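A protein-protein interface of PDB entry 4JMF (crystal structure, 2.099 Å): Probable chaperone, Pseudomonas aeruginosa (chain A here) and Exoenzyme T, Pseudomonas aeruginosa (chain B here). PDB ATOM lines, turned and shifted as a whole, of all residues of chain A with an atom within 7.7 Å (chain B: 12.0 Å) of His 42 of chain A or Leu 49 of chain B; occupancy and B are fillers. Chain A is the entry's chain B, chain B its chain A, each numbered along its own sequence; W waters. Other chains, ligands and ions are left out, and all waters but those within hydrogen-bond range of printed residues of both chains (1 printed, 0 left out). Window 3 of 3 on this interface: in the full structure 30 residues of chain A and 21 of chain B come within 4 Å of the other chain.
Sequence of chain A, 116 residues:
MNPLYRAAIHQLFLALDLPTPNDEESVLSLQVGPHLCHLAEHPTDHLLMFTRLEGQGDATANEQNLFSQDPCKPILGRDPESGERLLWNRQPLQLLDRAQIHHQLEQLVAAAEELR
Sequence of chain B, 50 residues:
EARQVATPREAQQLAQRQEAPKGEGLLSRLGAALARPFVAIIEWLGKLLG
His 42 of chain A touches one residue of chain B. Of chain B, only Leu 49 (3.6 Å) comes within 4 Å of Ala 40 of chain A. Glu 41 of chain A touches none of the printed residues of chain B. No residue of chain B comes within 4 Å of Pro 43 of chain A. No residue of chain B comes within 4 Å of Thr 44 of chain A. No residue of chain B comes within 4 Å of His 46 of chain A. Of chain B, only Leu 49 (3.8 Å) comes within 4 Å of Leu 48 of chain A. Of the printed residues of chain A, Leu 45 of chain B touches His 38 (3.6 Å) and Phe 50 (3.6 Å). Of the printed residues of chain B, Val 27 of chain A touches Leu 49 (3.9 Å). The nearest residue of chain A that does not touch Leu 49 of chain B is Phe 50 of chain A (4.5 Å). The nearest printed residue of chain B that does not touch Phe 50 of chain A is Leu 49 of chain B (4.5 Å).
Water W1 lies within hydrogen-bond range of O of Ile 42 of chain B (2.7 Å) and OG of Ser 26 of chain A (3.0 Å).
Among the printed residues, merely in contact across the chains: Val 27 of chain A with Leu 49 of chain B (3.9 Å), His 38 of chain A with Leu 45 of chain B (3.6 Å), Ala 40 of chain A with Leu 49 of chain B (3.6 Å), Leu 48 of chain A with Leu 49 of chain B (3.8 Å), Phe 50 of chain A with Leu 45 of chain B (3.6 Å) and Leu 86 of chain A with Leu 48 of chain B (3.9 Å).
Hydrophobic or aromatic side chains of chain A that line the printed part of chain B: Val 27, His 38, Ala 40, His 42, Leu 48, Phe 50 and Leu 86. Printed residues of chain B that touch a printed residue of chain A: Leu 45, Leu 48 and Leu 49. Among the printed residues, 7 pairs touch across the chains. Among the printed residues, no Asp or Glu carboxylate lies within 4 Å of a Lys or Arg side-chain nitrogen of the other chain.
O of Leu 49 of chain B lies within hydrogen-bond range of NE2 of His 42 of chain A (2.9 Å).
The side-chain hydroxyl (OH) of Tyr 5 of chain A lies close to the backbone NH (N) of Ala 40 of chain A. N of His 38 of chain A is in hydrogen-bond range of O of Phe 50 of chain A, at 2.8 Å. The backbone NH (N) of Leu 48 of chain A sits at hydrogen-bond distance from the backbone carbonyl oxygen (O) of Ala 40 of chain A, at 2.8 Å. The guanidinium group (NH1) of Arg 90 of chain A lies close to the backbone carbonyl oxygen (O) of His 42 of chain A (3.2 Å).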
ATOM      1  N   TYR A   5     -16.469  19.346  28.893  1.00  0.00           N
ATOM      2  CA  TYR A   5     -17.238  18.806  27.775  1.00  0.00           C
ATOM      3  C   TYR A   5     -16.363  18.771  26.524  1.00  0.00           C
ATOM      4  O   TYR A   5     -16.338  17.767  25.804  1.00  0.00           O
ATOM      5  CB  TYR A   5     -18.522  19.615  27.530  1.00  0.00           C
ATOM      6  CG  TYR A   5     -19.325  19.142  26.337  1.00  0.00           C
ATOM      7  CD1 TYR A   5     -20.148  18.030  26.433  1.00  0.00           C
ATOM      8  CD2 TYR A   5     -19.265  19.808  25.120  1.00  0.00           C
ATOM      9  CE1 TYR A   5     -20.880  17.588  25.348  1.00  0.00           C
ATOM     10  CE2 TYR A   5     -19.992  19.374  24.027  1.00  0.00           C
ATOM     11  CZ  TYR A   5     -20.801  18.260  24.152  1.00  0.00           C
ATOM     12  OH  TYR A   5     -21.546  17.808  23.076  1.00  0.00           O
ATOM     13  N   SER A  26     -23.324  24.427  21.165  1.00  0.00           N
ATOM     14  CA  SER A  26     -24.470  23.562  20.923  1.00  0.00           C
ATOM     15  C   SER A  26     -24.112  22.157  20.420  1.00  0.00           C
ATOM     16  O   SER A  26     -23.198  21.493  20.929  1.00  0.00           O
ATOM     17  CB  SER A  26     -25.469  24.221  19.951  1.00  0.00           C
ATOM     18  OG  SER A  26     -25.033  24.116  18.592  1.00  0.00           O
ATOM     19  N   VAL A  27     -24.853  21.737  19.399  1.00  0.00           N
ATOM     20  CA  VAL A  27     -24.993  20.338  19.041  1.00  0.00           C
ATOM     21  C   VAL A  27     -24.010  19.904  17.971  1.00  0.00           C
ATOM     22  O   VAL A  27     -23.954  20.507  16.887  1.00  0.00           O
ATOM     23  CB  VAL A  27     -26.425  20.079  18.546  1.00  0.00           C
ATOM     24  CG1 VAL A  27     -26.616  18.619  18.202  1.00  0.00           C
ATOM     25  CG2 VAL A  27     -27.423  20.512  19.608  1.00  0.00           C
ATOM     26  N   HIS A  38     -26.570  12.909  17.390  1.00  0.00           N
ATOM     27  CA  HIS A  38     -26.254  14.239  17.911  1.00  0.00           C
ATOM     28  C   HIS A  38     -25.720  14.138  19.344  1.00  0.00           C
ATOM     29  O   HIS A  38     -26.120  13.238  20.087  1.00  0.00           O
ATOM     30  CB  HIS A  38     -27.506  15.129  17.902  1.00  0.00           C
ATOM     31  CG  HIS A  38     -28.317  15.011  16.651  1.00  0.00           C
ATOM     32  ND1 HIS A  38     -28.041  15.739  15.512  1.00  0.00           N
ATOM     33  CD2 HIS A  38     -29.393  14.242  16.356  1.00  0.00           C
ATOM     34  CE1 HIS A  38     -28.913  15.423  14.569  1.00  0.00           C
ATOM     35  NE2 HIS A  38     -29.745  14.519  15.055  1.00  0.00           N
ATOM     36  N   LEU A  39     -24.839  15.069  19.722  1.00  0.00           N
ATOM     37  CA  LEU A  39     -24.213  15.071  21.035  1.00  0.00           C
ATOM     38  C   LEU A  39     -24.383  16.462  21.585  1.00  0.00           C
ATOM     39  O   LEU A  39     -24.233  17.436  20.850  1.00  0.00           O
ATOM     40  CB  LEU A  39     -22.711  14.796  20.925  1.00  0.00           C
ATOM     41  CG  LEU A  39     -22.241  13.812  19.862  1.00  0.00           C
ATOM     42  CD1 LEU A  39     -20.697  13.773  19.815  1.00  0.00           C
ATOM     43  CD2 LEU A  39     -22.792  12.459  20.139  1.00  0.00           C
ATOM     44  N   ALA A  40     -24.697  16.568  22.870  1.00  0.00           N
ATOM     45  CA  ALA A  40     -24.825  17.879  23.475  1.00  0.00           C
ATOM     46  C   ALA A  40     -24.554  17.762  24.950  1.00  0.00           C
ATOM     47  O   ALA A  40     -24.744  16.697  25.530  1.00  0.00           O
ATOM     48  CB  ALA A  40     -26.237  18.429  23.250  1.00  0.00           C
ATOM     49  N   GLU A  41     -24.119  18.852  25.563  1.00  0.00           N
ATOM     50  CA  GLU A  41     -24.045  18.884  27.012  1.00  0.00           C
ATOM     51  C   GLU A  41     -25.441  19.181  27.565  1.00  0.00           C
ATOM     52  O   GLU A  41     -25.969  20.274  27.371  1.00  0.00           O
ATOM     53  CB  GLU A  41     -23.080  19.959  27.491  1.00  0.00           C
ATOM     54  CG  GLU A  41     -22.897  19.903  28.998  1.00  0.00           C
ATOM     55  CD  GLU A  41     -21.955  20.965  29.532  1.00  0.00           C
ATOM     56  OE1 GLU A  41     -21.619  21.922  28.793  1.00  0.00           O
ATOM     57  OE2 GLU A  41     -21.556  20.840  30.712  1.00  0.00           O
ATOM     58  N   HIS A  42     -26.036  18.222  28.267  1.00  0.00           N
ATOM     59  CA  HIS A  42     -27.428  18.391  28.685  1.00  0.00           C
ATOM     60  C   HIS A  42     -27.793  17.376  29.743  1.00  0.00           C
ATOM     61  O   HIS A  42     -27.834  16.181  29.458  1.00  0.00           O
ATOM     62  CB  HIS A  42     -28.359  18.225  27.481  1.00  0.00           C
ATOM     63  CG  HIS A  42     -29.777  18.626  27.751  1.00  0.00           C
ATOM     64  ND1 HIS A  42     -30.725  17.742  28.221  1.00  0.00           N
ATOM     65  CD2 HIS A  42     -30.412  19.815  27.607  1.00  0.00           C
ATOM     66  CE1 HIS A  42     -31.886  18.365  28.350  1.00  0.00           C
ATOM     67  NE2 HIS A  42     -31.722  19.625  27.985  1.00  0.00           N
ATOM     68  N   PRO A  43     -28.013  17.832  30.986  1.00  0.00           N
ATOM     69  CA  PRO A  43     -27.788  19.205  31.453  1.00  0.00           C
ATOM     70  C   PRO A  43     -26.306  19.403  31.630  1.00  0.00           C
ATOM     71  O   PRO A  43     -25.519  18.555  31.179  1.00  0.00           O
ATOM     72  CB  PRO A  43     -28.462  19.223  32.831  1.00  0.00           C
ATOM     73  CG  PRO A  43     -28.340  17.781  33.309  1.00  0.00           C
ATOM     74  CD  PRO A  43     -28.460  16.934  32.067  1.00  0.00           C
ATOM     75  N   THR A  44     -25.929  20.505  32.266  1.00  0.00           N
ATOM     76  CA  THR A  44     -24.535  20.783  32.569  1.00  0.00           C
ATOM     77  C   THR A  44     -23.855  19.553  33.172  1.00  0.00           C
ATOM     78  O   THR A  44     -24.451  18.839  33.993  1.00  0.00           O
ATOM     79  CB  THR A  44     -24.446  21.986  33.509  1.00  0.00           C
ATOM     80  OG1 THR A  44     -25.097  23.084  32.869  1.00  0.00           O
ATOM     81  CG2 THR A  44     -22.991  22.377  33.779  1.00  0.00           C
ATOM     82  N   ASP A  45     -22.634  19.286  32.707  1.00  0.00           N
ATOM     83  CA  ASP A  45     -21.806  18.166  33.179  1.00  0.00           C
ATOM     84  C   ASP A  45     -22.308  16.775  32.810  1.00  0.00           C
ATOM     85  O   ASP A  45     -21.787  15.778  33.318  1.00  0.00           O
ATOM     86  CB  ASP A  45     -21.548  18.262  34.690  1.00  0.00           C
ATOM     87  CG  ASP A  45     -20.725  19.480  35.058  1.00  0.00           C
ATOM     88  OD1 ASP A  45     -19.723  19.758  34.360  1.00  0.00           O
ATOM     89  OD2 ASP A  45     -21.094  20.168  36.031  1.00  0.00           O
ATOM     90  N   HIS A  46     -23.295  16.700  31.918  1.00  0.00           N
ATOM     91  CA  HIS A  46     -23.687  15.407  31.339  1.00  0.00           C
ATOM     92  C   HIS A  46     -23.613  15.443  29.821  1.00  0.00           C
ATOM     93  O   HIS A  46     -23.781  16.496  29.207  1.00  0.00           O
ATOM     94  CB  HIS A  46     -25.104  15.001  31.760  1.00  0.00           C
ATOM     95  CG  HIS A  46     -25.268  14.791  33.230  1.00  0.00           C
ATOM     96  ND1 HIS A  46     -25.197  15.826  34.138  1.00  0.00           N
ATOM     97  CD2 HIS A  46     -25.520  13.672  33.949  1.00  0.00           C
ATOM     98  CE1 HIS A  46     -25.400  15.354  35.353  1.00  0.00           C
ATOM     99  NE2 HIS A  46     -25.584  14.049  35.269  1.00  0.00           N
ATOM    100  N   LEU A  47     -23.347  14.292  29.212  1.00  0.00           N
ATOM    101  CA  LEU A  47     -23.284  14.207  27.756  1.00  0.00           C
ATOM    102  C   LEU A  47     -24.498  13.439  27.263  1.00  0.00           C
ATOM    103  O   LEU A  47     -24.674  12.260  27.598  1.00  0.00           O
ATOM    104  CB  LEU A  47     -22.012  13.481  27.304  1.00  0.00           C
ATOM    105  CG  LEU A  47     -21.945  13.079  25.826  1.00  0.00           C
ATOM    106  CD1 LEU A  47     -22.004  14.302  24.925  1.00  0.00           C
ATOM    107  CD2 LEU A  47     -20.665  12.340  25.556  1.00  0.00           C
ATOM    108  N   LEU A  48     -25.326  14.109  26.470  1.00  0.00           N
ATOM    109  CA  LEU A  48     -26.519  13.488  25.911  1.00  0.00           C
ATOM    110  C   LEU A  48     -26.230  13.093  24.473  1.00  0.00           C
ATOM    111  O   LEU A  48     -25.780  13.924  23.694  1.00  0.00           O
ATOM    112  CB  LEU A  48     -27.678  14.484  25.949  1.00  0.00           C
ATOM    113  CG  LEU A  48     -29.023  14.061  25.363  1.00  0.00           C
ATOM    114  CD1 LEU A  48     -29.726  13.045  26.282  1.00  0.00           C
ATOM    115  CD2 LEU A  48     -29.902  15.300  25.123  1.00  0.00           C
ATOM    116  N   MET A  49     -26.461  11.827  24.126  1.00  0.00           N
ATOM    117  CA  MET A  49     -26.351  11.393  22.734  1.00  0.00           C
ATOM    118  C   MET A  49     -27.715  10.928  22.264  1.00  0.00           C
ATOM    119  O   MET A  49     -28.420  10.221  22.992  1.00  0.00           O
ATOM    120  CB  MET A  49     -25.370  10.224  22.593  1.00  0.00           C
ATOM    121  CG  MET A  49     -23.960  10.509  23.075  1.00  0.00           C
ATOM    122  SD  MET A  49     -22.885   9.168  22.560  1.00  0.00           S
ATOM    123  CE  MET A  49     -21.312   9.682  23.245  1.00  0.00           C
ATOM    124  N   PHE A  50     -28.093  11.287  21.043  1.00  0.00           N
ATOM    125  CA  PHE A  50     -29.397  10.834  20.563  1.00  0.00           C
ATOM    126  C   PHE A  50     -29.484  10.776  19.056  1.00  0.00           C
ATOM    127  O   PHE A  50     -28.681  11.390  18.352  1.00  0.00           O
ATOM    128  CB  PHE A  50     -30.531  11.707  21.135  1.00  0.00           C
ATOM    129  CG  PHE A  50     -30.421  13.168  20.779  1.00  0.00           C
ATOM    130  CD1 PHE A  50     -31.177  13.704  19.746  1.00  0.00           C
ATOM    131  CD2 PHE A  50     -29.581  14.014  21.498  1.00  0.00           C
ATOM    132  CE1 PHE A  50     -31.080  15.064  19.426  1.00  0.00           C
ATOM    133  CE2 PHE A  50     -29.479  15.372  21.185  1.00  0.00           C
ATOM    134  CZ  PHE A  50     -30.229  15.893  20.151  1.00  0.00           C
ATOM    135  N   LEU A  86     -37.201  10.210  19.645  1.00  0.00           N
ATOM    136  CA  LEU A  86     -35.747  10.289  19.827  1.00  0.00           C
ATOM    137  C   LEU A  86     -35.256   9.130  20.682  1.00  0.00           C
ATOM    138  O   LEU A  86     -35.784   8.883  21.780  1.00  0.00           O
ATOM    139  CB  LEU A  86     -35.354  11.617  20.484  1.00  0.00           C
ATOM    140  CG  LEU A  86     -35.789  12.940  19.843  1.00  0.00           C
ATOM    141  CD1 LEU A  86     -35.246  14.118  20.640  1.00  0.00           C
ATOM    142  CD2 LEU A  86     -35.331  13.039  18.389  1.00  0.00           C
ATOM    143  N   TRP A  88     -32.169   7.899  22.864  1.00  0.00           N
ATOM    144  CA  TRP A  88     -31.152   8.702  23.539  1.00  0.00           C
ATOM    145  C   TRP A  88     -30.530   7.996  24.715  1.00  0.00           C
ATOM    146  O   TRP A  88     -31.142   7.112  25.333  1.00  0.00           O
ATOM    147  CB  TRP A  88     -31.749  10.023  24.038  1.00  0.00           C
ATOM    148  CG  TRP A  88     -32.844   9.839  25.058  1.00  0.00           C
ATOM    149  CD1 TRP A  88     -34.168   9.594  24.803  1.00  0.00           C
ATOM    150  CD2 TRP A  88     -32.715   9.882  26.488  1.00  0.00           C
ATOM    151  NE1 TRP A  88     -34.872   9.496  25.983  1.00  0.00           N
ATOM    152  CE2 TRP A  88     -34.003   9.661  27.033  1.00  0.00           C
ATOM    153  CE3 TRP A  88     -31.638  10.086  27.364  1.00  0.00           C
ATOM    154  CZ2 TRP A  88     -34.242   9.641  28.412  1.00  0.00           C
ATOM    155  CZ3 TRP A  88     -31.878  10.069  28.740  1.00  0.00           C
ATOM    156  CH2 TRP A  88     -33.174   9.848  29.248  1.00  0.00           C
ATOM    157  N   ASN A  89     -29.304   8.398  25.041  1.00  0.00           N
ATOM    158  CA  ASN A  89     -28.731   8.005  26.323  1.00  0.00           C
ATOM    159  C   ASN A  89     -27.929   9.158  26.907  1.00  0.00           C
ATOM    160  O   ASN A  89     -27.778  10.196  26.256  1.00  0.00           O
ATOM    161  CB  ASN A  89     -27.950   6.688  26.231  1.00  0.00           C
ATOM    162  CG  ASN A  89     -26.781   6.754  25.263  1.00  0.00           C
ATOM    163  OD1 ASN A  89     -26.323   7.839  24.874  1.00  0.00           O
ATOM    164  ND2 ASN A  89     -26.277   5.581  24.880  1.00  0.00           N
ATOM    165  N   ARG A  90     -27.461   9.016  28.142  1.00  0.00           N
ATOM    166  CA  ARG A  90     -26.768  10.125  28.795  1.00  0.00           C
ATOM    167  C   ARG A  90     -25.772   9.620  29.824  1.00  0.00           C
ATOM    168  O   ARG A  90     -26.042   8.640  30.527  1.00  0.00           O
ATOM    169  CB  ARG A  90     -27.767  11.063  29.475  1.00  0.00           C
ATOM    170  CG  ARG A  90     -27.094  12.186  30.259  1.00  0.00           C
ATOM    171  CD  ARG A  90     -27.997  13.389  30.370  1.00  0.00           C
ATOM    172  NE  ARG A  90     -29.231  13.007  30.982  1.00  0.00           N
ATOM    173  CZ  ARG A  90     -30.401  13.607  30.809  1.00  0.00           C
ATOM    174  NH1 ARG A  90     -30.553  14.688  30.030  1.00  0.00           N
ATOM    175  NH2 ARG A  90     -31.426  13.093  31.448  1.00  0.00           N
ATOM    176  N   GLN A  91     -24.617  10.281  29.900  1.00  0.00           N
ATOM    177  CA  GLN A  91     -23.610   9.915  30.879  1.00  0.00           C
ATOM    178  C   GLN A  91     -23.046  11.167  31.507  1.00  0.00           C
ATOM    179  O   GLN A  91     -22.972  12.205  30.857  1.00  0.00           O
ATOM    180  CB  GLN A  91     -22.490   9.097  30.228  1.00  0.00           C
ATOM    181  CG  GLN A  91     -22.907   7.684  29.812  1.00  0.00           C
ATOM    182  CD  GLN A  91     -22.929   6.702  30.984  1.00  0.00           C
ATOM    183  OE1 GLN A  91     -21.924   6.042  31.282  1.00  0.00           O
ATOM    184  NE2 GLN A  91     -24.077   6.600  31.649  1.00  0.00           N
ATOM    185  N   LEU A  93     -20.133  13.562  32.658  1.00  0.00           N
ATOM    186  CA  LEU A  93     -18.766  13.726  32.153  1.00  0.00           C
ATOM    187  C   LEU A  93     -17.707  13.110  33.081  1.00  0.00           C
ATOM    188  O   LEU A  93     -16.656  12.667  32.618  1.00  0.00           O
ATOM    189  CB  LEU A  93     -18.470  15.206  31.892  1.00  0.00           C
ATOM    190  CG  LEU A  93     -19.308  15.894  30.814  1.00  0.00           C
ATOM    191  CD1 LEU A  93     -18.977  17.385  30.726  1.00  0.00           C
ATOM    192  CD2 LEU A  93     -19.111  15.232  29.454  1.00  0.00           C
ATOM    193  N   PRO B  37     -25.733  18.598   9.141  1.00  0.00           N
ATOM    194  CA  PRO B  37     -27.158  18.506   8.796  1.00  0.00           C
ATOM    195  C   PRO B  37     -27.778  19.889   8.631  1.00  0.00           C
ATOM    196  O   PRO B  37     -27.122  20.862   9.013  1.00  0.00           O
ATOM    197  CB  PRO B  37     -27.764  17.770  10.002  1.00  0.00           C
ATOM    198  CG  PRO B  37     -26.831  18.046  11.144  1.00  0.00           C
ATOM    199  CD  PRO B  37     -25.468  18.351  10.573  1.00  0.00           C
ATOM    200  N   VAL B  39     -29.290  23.408   8.915  1.00  0.00           N
ATOM    201  CA  VAL B  39     -29.234  24.404   9.970  1.00  0.00           C
ATOM    202  C   VAL B  39     -30.500  24.343  10.804  1.00  0.00           C
ATOM    203  O   VAL B  39     -30.458  24.485  12.025  1.00  0.00           O
ATOM    204  CB  VAL B  39     -29.079  25.804   9.367  1.00  0.00           C
ATOM    205  CG1 VAL B  39     -29.146  26.876  10.454  1.00  0.00           C
ATOM    206  CG2 VAL B  39     -27.769  25.887   8.606  1.00  0.00           C
ATOM    207  N   ALA B  40     -31.625  24.098  10.137  1.00  0.00           N
ATOM    208  CA  ALA B  40     -32.916  24.022  10.795  1.00  0.00           C
ATOM    209  C   ALA B  40     -32.959  22.959  11.890  1.00  0.00           C
ATOM    210  O   ALA B  40     -33.622  23.143  12.915  1.00  0.00           O
ATOM    211  CB  ALA B  40     -34.005  23.757   9.777  1.00  0.00           C
ATOM    212  N   ILE B  41     -32.279  21.841  11.667  1.00  0.00           N
ATOM    213  CA  ILE B  41     -32.266  20.778  12.669  1.00  0.00           C
ATOM    214  C   ILE B  41     -31.470  21.255  13.878  1.00  0.00           C
ATOM    215  O   ILE B  41     -31.917  21.126  15.024  1.00  0.00           O
ATOM    216  CB  ILE B  41     -31.650  19.480  12.117  1.00  0.00           C
ATOM    217  CG1 ILE B  41     -32.528  18.907  11.002  1.00  0.00           C
ATOM    218  CG2 ILE B  41     -31.483  18.446  13.223  1.00  0.00           C
ATOM    219  CD1 ILE B  41     -31.833  17.847  10.183  1.00  0.00           C
ATOM    220  N   ILE B  42     -30.309  21.844  13.601  1.00  0.00           N
ATOM    221  CA  ILE B  42     -29.395  22.309  14.646  1.00  0.00           C
ATOM    222  C   ILE B  42     -30.039  23.385  15.515  1.00  0.00           C
ATOM    223  O   ILE B  42     -29.998  23.314  16.752  1.00  0.00           O
ATOM    224  CB  ILE B  42     -28.072  22.821  14.041  1.00  0.00           C
ATOM    225  CG1 ILE B  42     -27.416  21.707  13.223  1.00  0.00           C
ATOM    226  CG2 ILE B  42     -27.128  23.290  15.126  1.00  0.00           C
ATOM    227  CD1 ILE B  42     -27.452  20.369  13.924  1.00  0.00           C
ATOM    228  N   GLU B  43     -30.672  24.358  14.873  1.00  0.00           N
ATOM    229  CA  GLU B  43     -31.361  25.420  15.606  1.00  0.00           C
ATOM    230  C   GLU B  43     -32.537  24.902  16.436  1.00  0.00           C
ATOM    231  O   GLU B  43     -32.722  25.310  17.587  1.00  0.00           O
ATOM    232  CB  GLU B  43     -31.785  26.534  14.650  1.00  0.00           C
ATOM    233  CG  GLU B  43     -30.579  27.362  14.156  1.00  0.00           C
ATOM    234  CD  GLU B  43     -30.958  28.430  13.137  1.00  0.00           C
ATOM    235  OE1 GLU B  43     -32.169  28.580  12.833  1.00  0.00           O
ATOM    236  OE2 GLU B  43     -30.035  29.113  12.636  1.00  0.00           O
ATOM    237  N   TRP B  44     -33.322  23.994  15.860  1.00  0.00           N
ATOM    238  CA  TRP B  44     -34.435  23.393  16.589  1.00  0.00           C
ATOM    239  C   TRP B  44     -33.922  22.596  17.798  1.00  0.00           C
ATOM    240  O   TRP B  44     -34.447  22.715  18.909  1.00  0.00           O
ATOM    241  CB  TRP B  44     -35.262  22.485  15.665  1.00  0.00           C
ATOM    242  CG  TRP B  44     -36.300  21.703  16.400  1.00  0.00           C
ATOM    243  CD1 TRP B  44     -37.428  22.194  16.985  1.00  0.00           C
ATOM    244  CD2 TRP B  44     -36.296  20.290  16.662  1.00  0.00           C
ATOM    245  NE1 TRP B  44     -38.134  21.175  17.583  1.00  0.00           N
ATOM    246  CE2 TRP B  44     -37.458  19.998  17.397  1.00  0.00           C
ATOM    247  CE3 TRP B  44     -35.431  19.247  16.326  1.00  0.00           C
ATOM    248  CZ2 TRP B  44     -37.770  18.706  17.816  1.00  0.00           C
ATOM    249  CZ3 TRP B  44     -35.747  17.961  16.738  1.00  0.00           C
ATOM    250  CH2 TRP B  44     -36.899  17.705  17.477  1.00  0.00           C
ATOM    251  N   LEU B  45     -32.901  21.780  17.571  1.00  0.00           N
ATOM    252  CA  LEU B  45     -32.321  20.997  18.654  1.00  0.00           C
ATOM    253  C   LEU B  45     -31.875  21.910  19.784  1.00  0.00           C
ATOM    254  O   LEU B  45     -32.053  21.574  20.943  1.00  0.00           O
ATOM    255  CB  LEU B  45     -31.163  20.114  18.152  1.00  0.00           C
ATOM    256  CG  LEU B  45     -31.590  18.918  17.300  1.00  0.00           C
ATOM    257  CD1 LEU B  45     -30.378  18.114  16.824  1.00  0.00           C
ATOM    258  CD2 LEU B  45     -32.592  18.009  18.044  1.00  0.00           C
ATOM    259  N   GLY B  46     -31.335  23.082  19.446  1.00  0.00           N
ATOM    260  CA  GLY B  46     -30.955  24.051  20.466  1.00  0.00           C
ATOM    261  C   GLY B  46     -32.131  24.558  21.281  1.00  0.00           C
ATOM    262  O   GLY B  46     -32.014  24.796  22.489  1.00  0.00           O
ATOM    263  N   LYS B  47     -33.277  24.736  20.635  1.00  0.00           N
ATOM    264  CA  LYS B  47     -34.457  25.176  21.373  1.00  0.00           C
ATOM    265  C   LYS B  47     -35.034  24.030  22.188  1.00  0.00           C
ATOM    266  O   LYS B  47     -35.531  24.234  23.292  1.00  0.00           O
ATOM    267  CB  LYS B  47     -35.522  25.758  20.426  1.00  0.00           C
ATOM    268  CG  LYS B  47     -35.220  27.180  19.931  1.00  0.00           C
ATOM    269  CD  LYS B  47     -36.287  27.655  18.939  1.00  0.00           C
ATOM    270  CE  LYS B  47     -35.771  28.801  18.046  1.00  0.00           C
ATOM    271  NZ  LYS B  47     -35.512  30.062  18.813  1.00  0.00           N
ATOM    272  N   LEU B  48     -34.973  22.819  21.650  1.00  0.00           N
ATOM    273  CA  LEU B  48     -35.489  21.667  22.375  1.00  0.00           C
ATOM    274  C   LEU B  48     -34.676  21.467  23.651  1.00  0.00           C
ATOM    275  O   LEU B  48     -35.227  21.241  24.722  1.00  0.00           O
ATOM    276  CB  LEU B  48     -35.426  20.414  21.496  1.00  0.00           C
ATOM    277  CG  LEU B  48     -35.741  19.073  22.160  1.00  0.00           C
ATOM    278  CD1 LEU B  48     -37.207  18.976  22.580  1.00  0.00           C
ATOM    279  CD2 LEU B  48     -35.393  17.949  21.204  1.00  0.00           C
ATOM    280  N   LEU B  49     -33.358  21.572  23.529  1.00  0.00           N
ATOM    281  CA  LEU B  49     -32.468  21.310  24.655  1.00  0.00           C
ATOM    282  C   LEU B  49     -32.466  22.446  25.673  1.00  0.00           C
ATOM    283  O   LEU B  49     -32.240  22.213  26.865  1.00  0.00           O
ATOM    284  CB  LEU B  49     -31.048  21.042  24.155  1.00  0.00           C
ATOM    285  CG  LEU B  49     -30.985  19.803  23.270  1.00  0.00           C
ATOM    286  CD1 LEU B  49     -29.588  19.616  22.694  1.00  0.00           C
ATOM    287  CD2 LEU B  49     -31.402  18.590  24.067  1.00  0.00           C
ATOM    288  N   GLY B  50     -32.717  23.667  25.212  1.00  0.00           N
ATOM    289  CA  GLY B  50     -32.873  24.796  26.120  1.00  0.00           C
ATOM    290  C   GLY B  50     -34.249  24.754  26.769  1.00  0.00           C
ATOM    291  O   GLY B  50     -34.518  25.447  27.755  1.00  0.00           O
HETATM  292  O   HOH W   1     -28.076  24.173  18.435  1.00  0.00           O
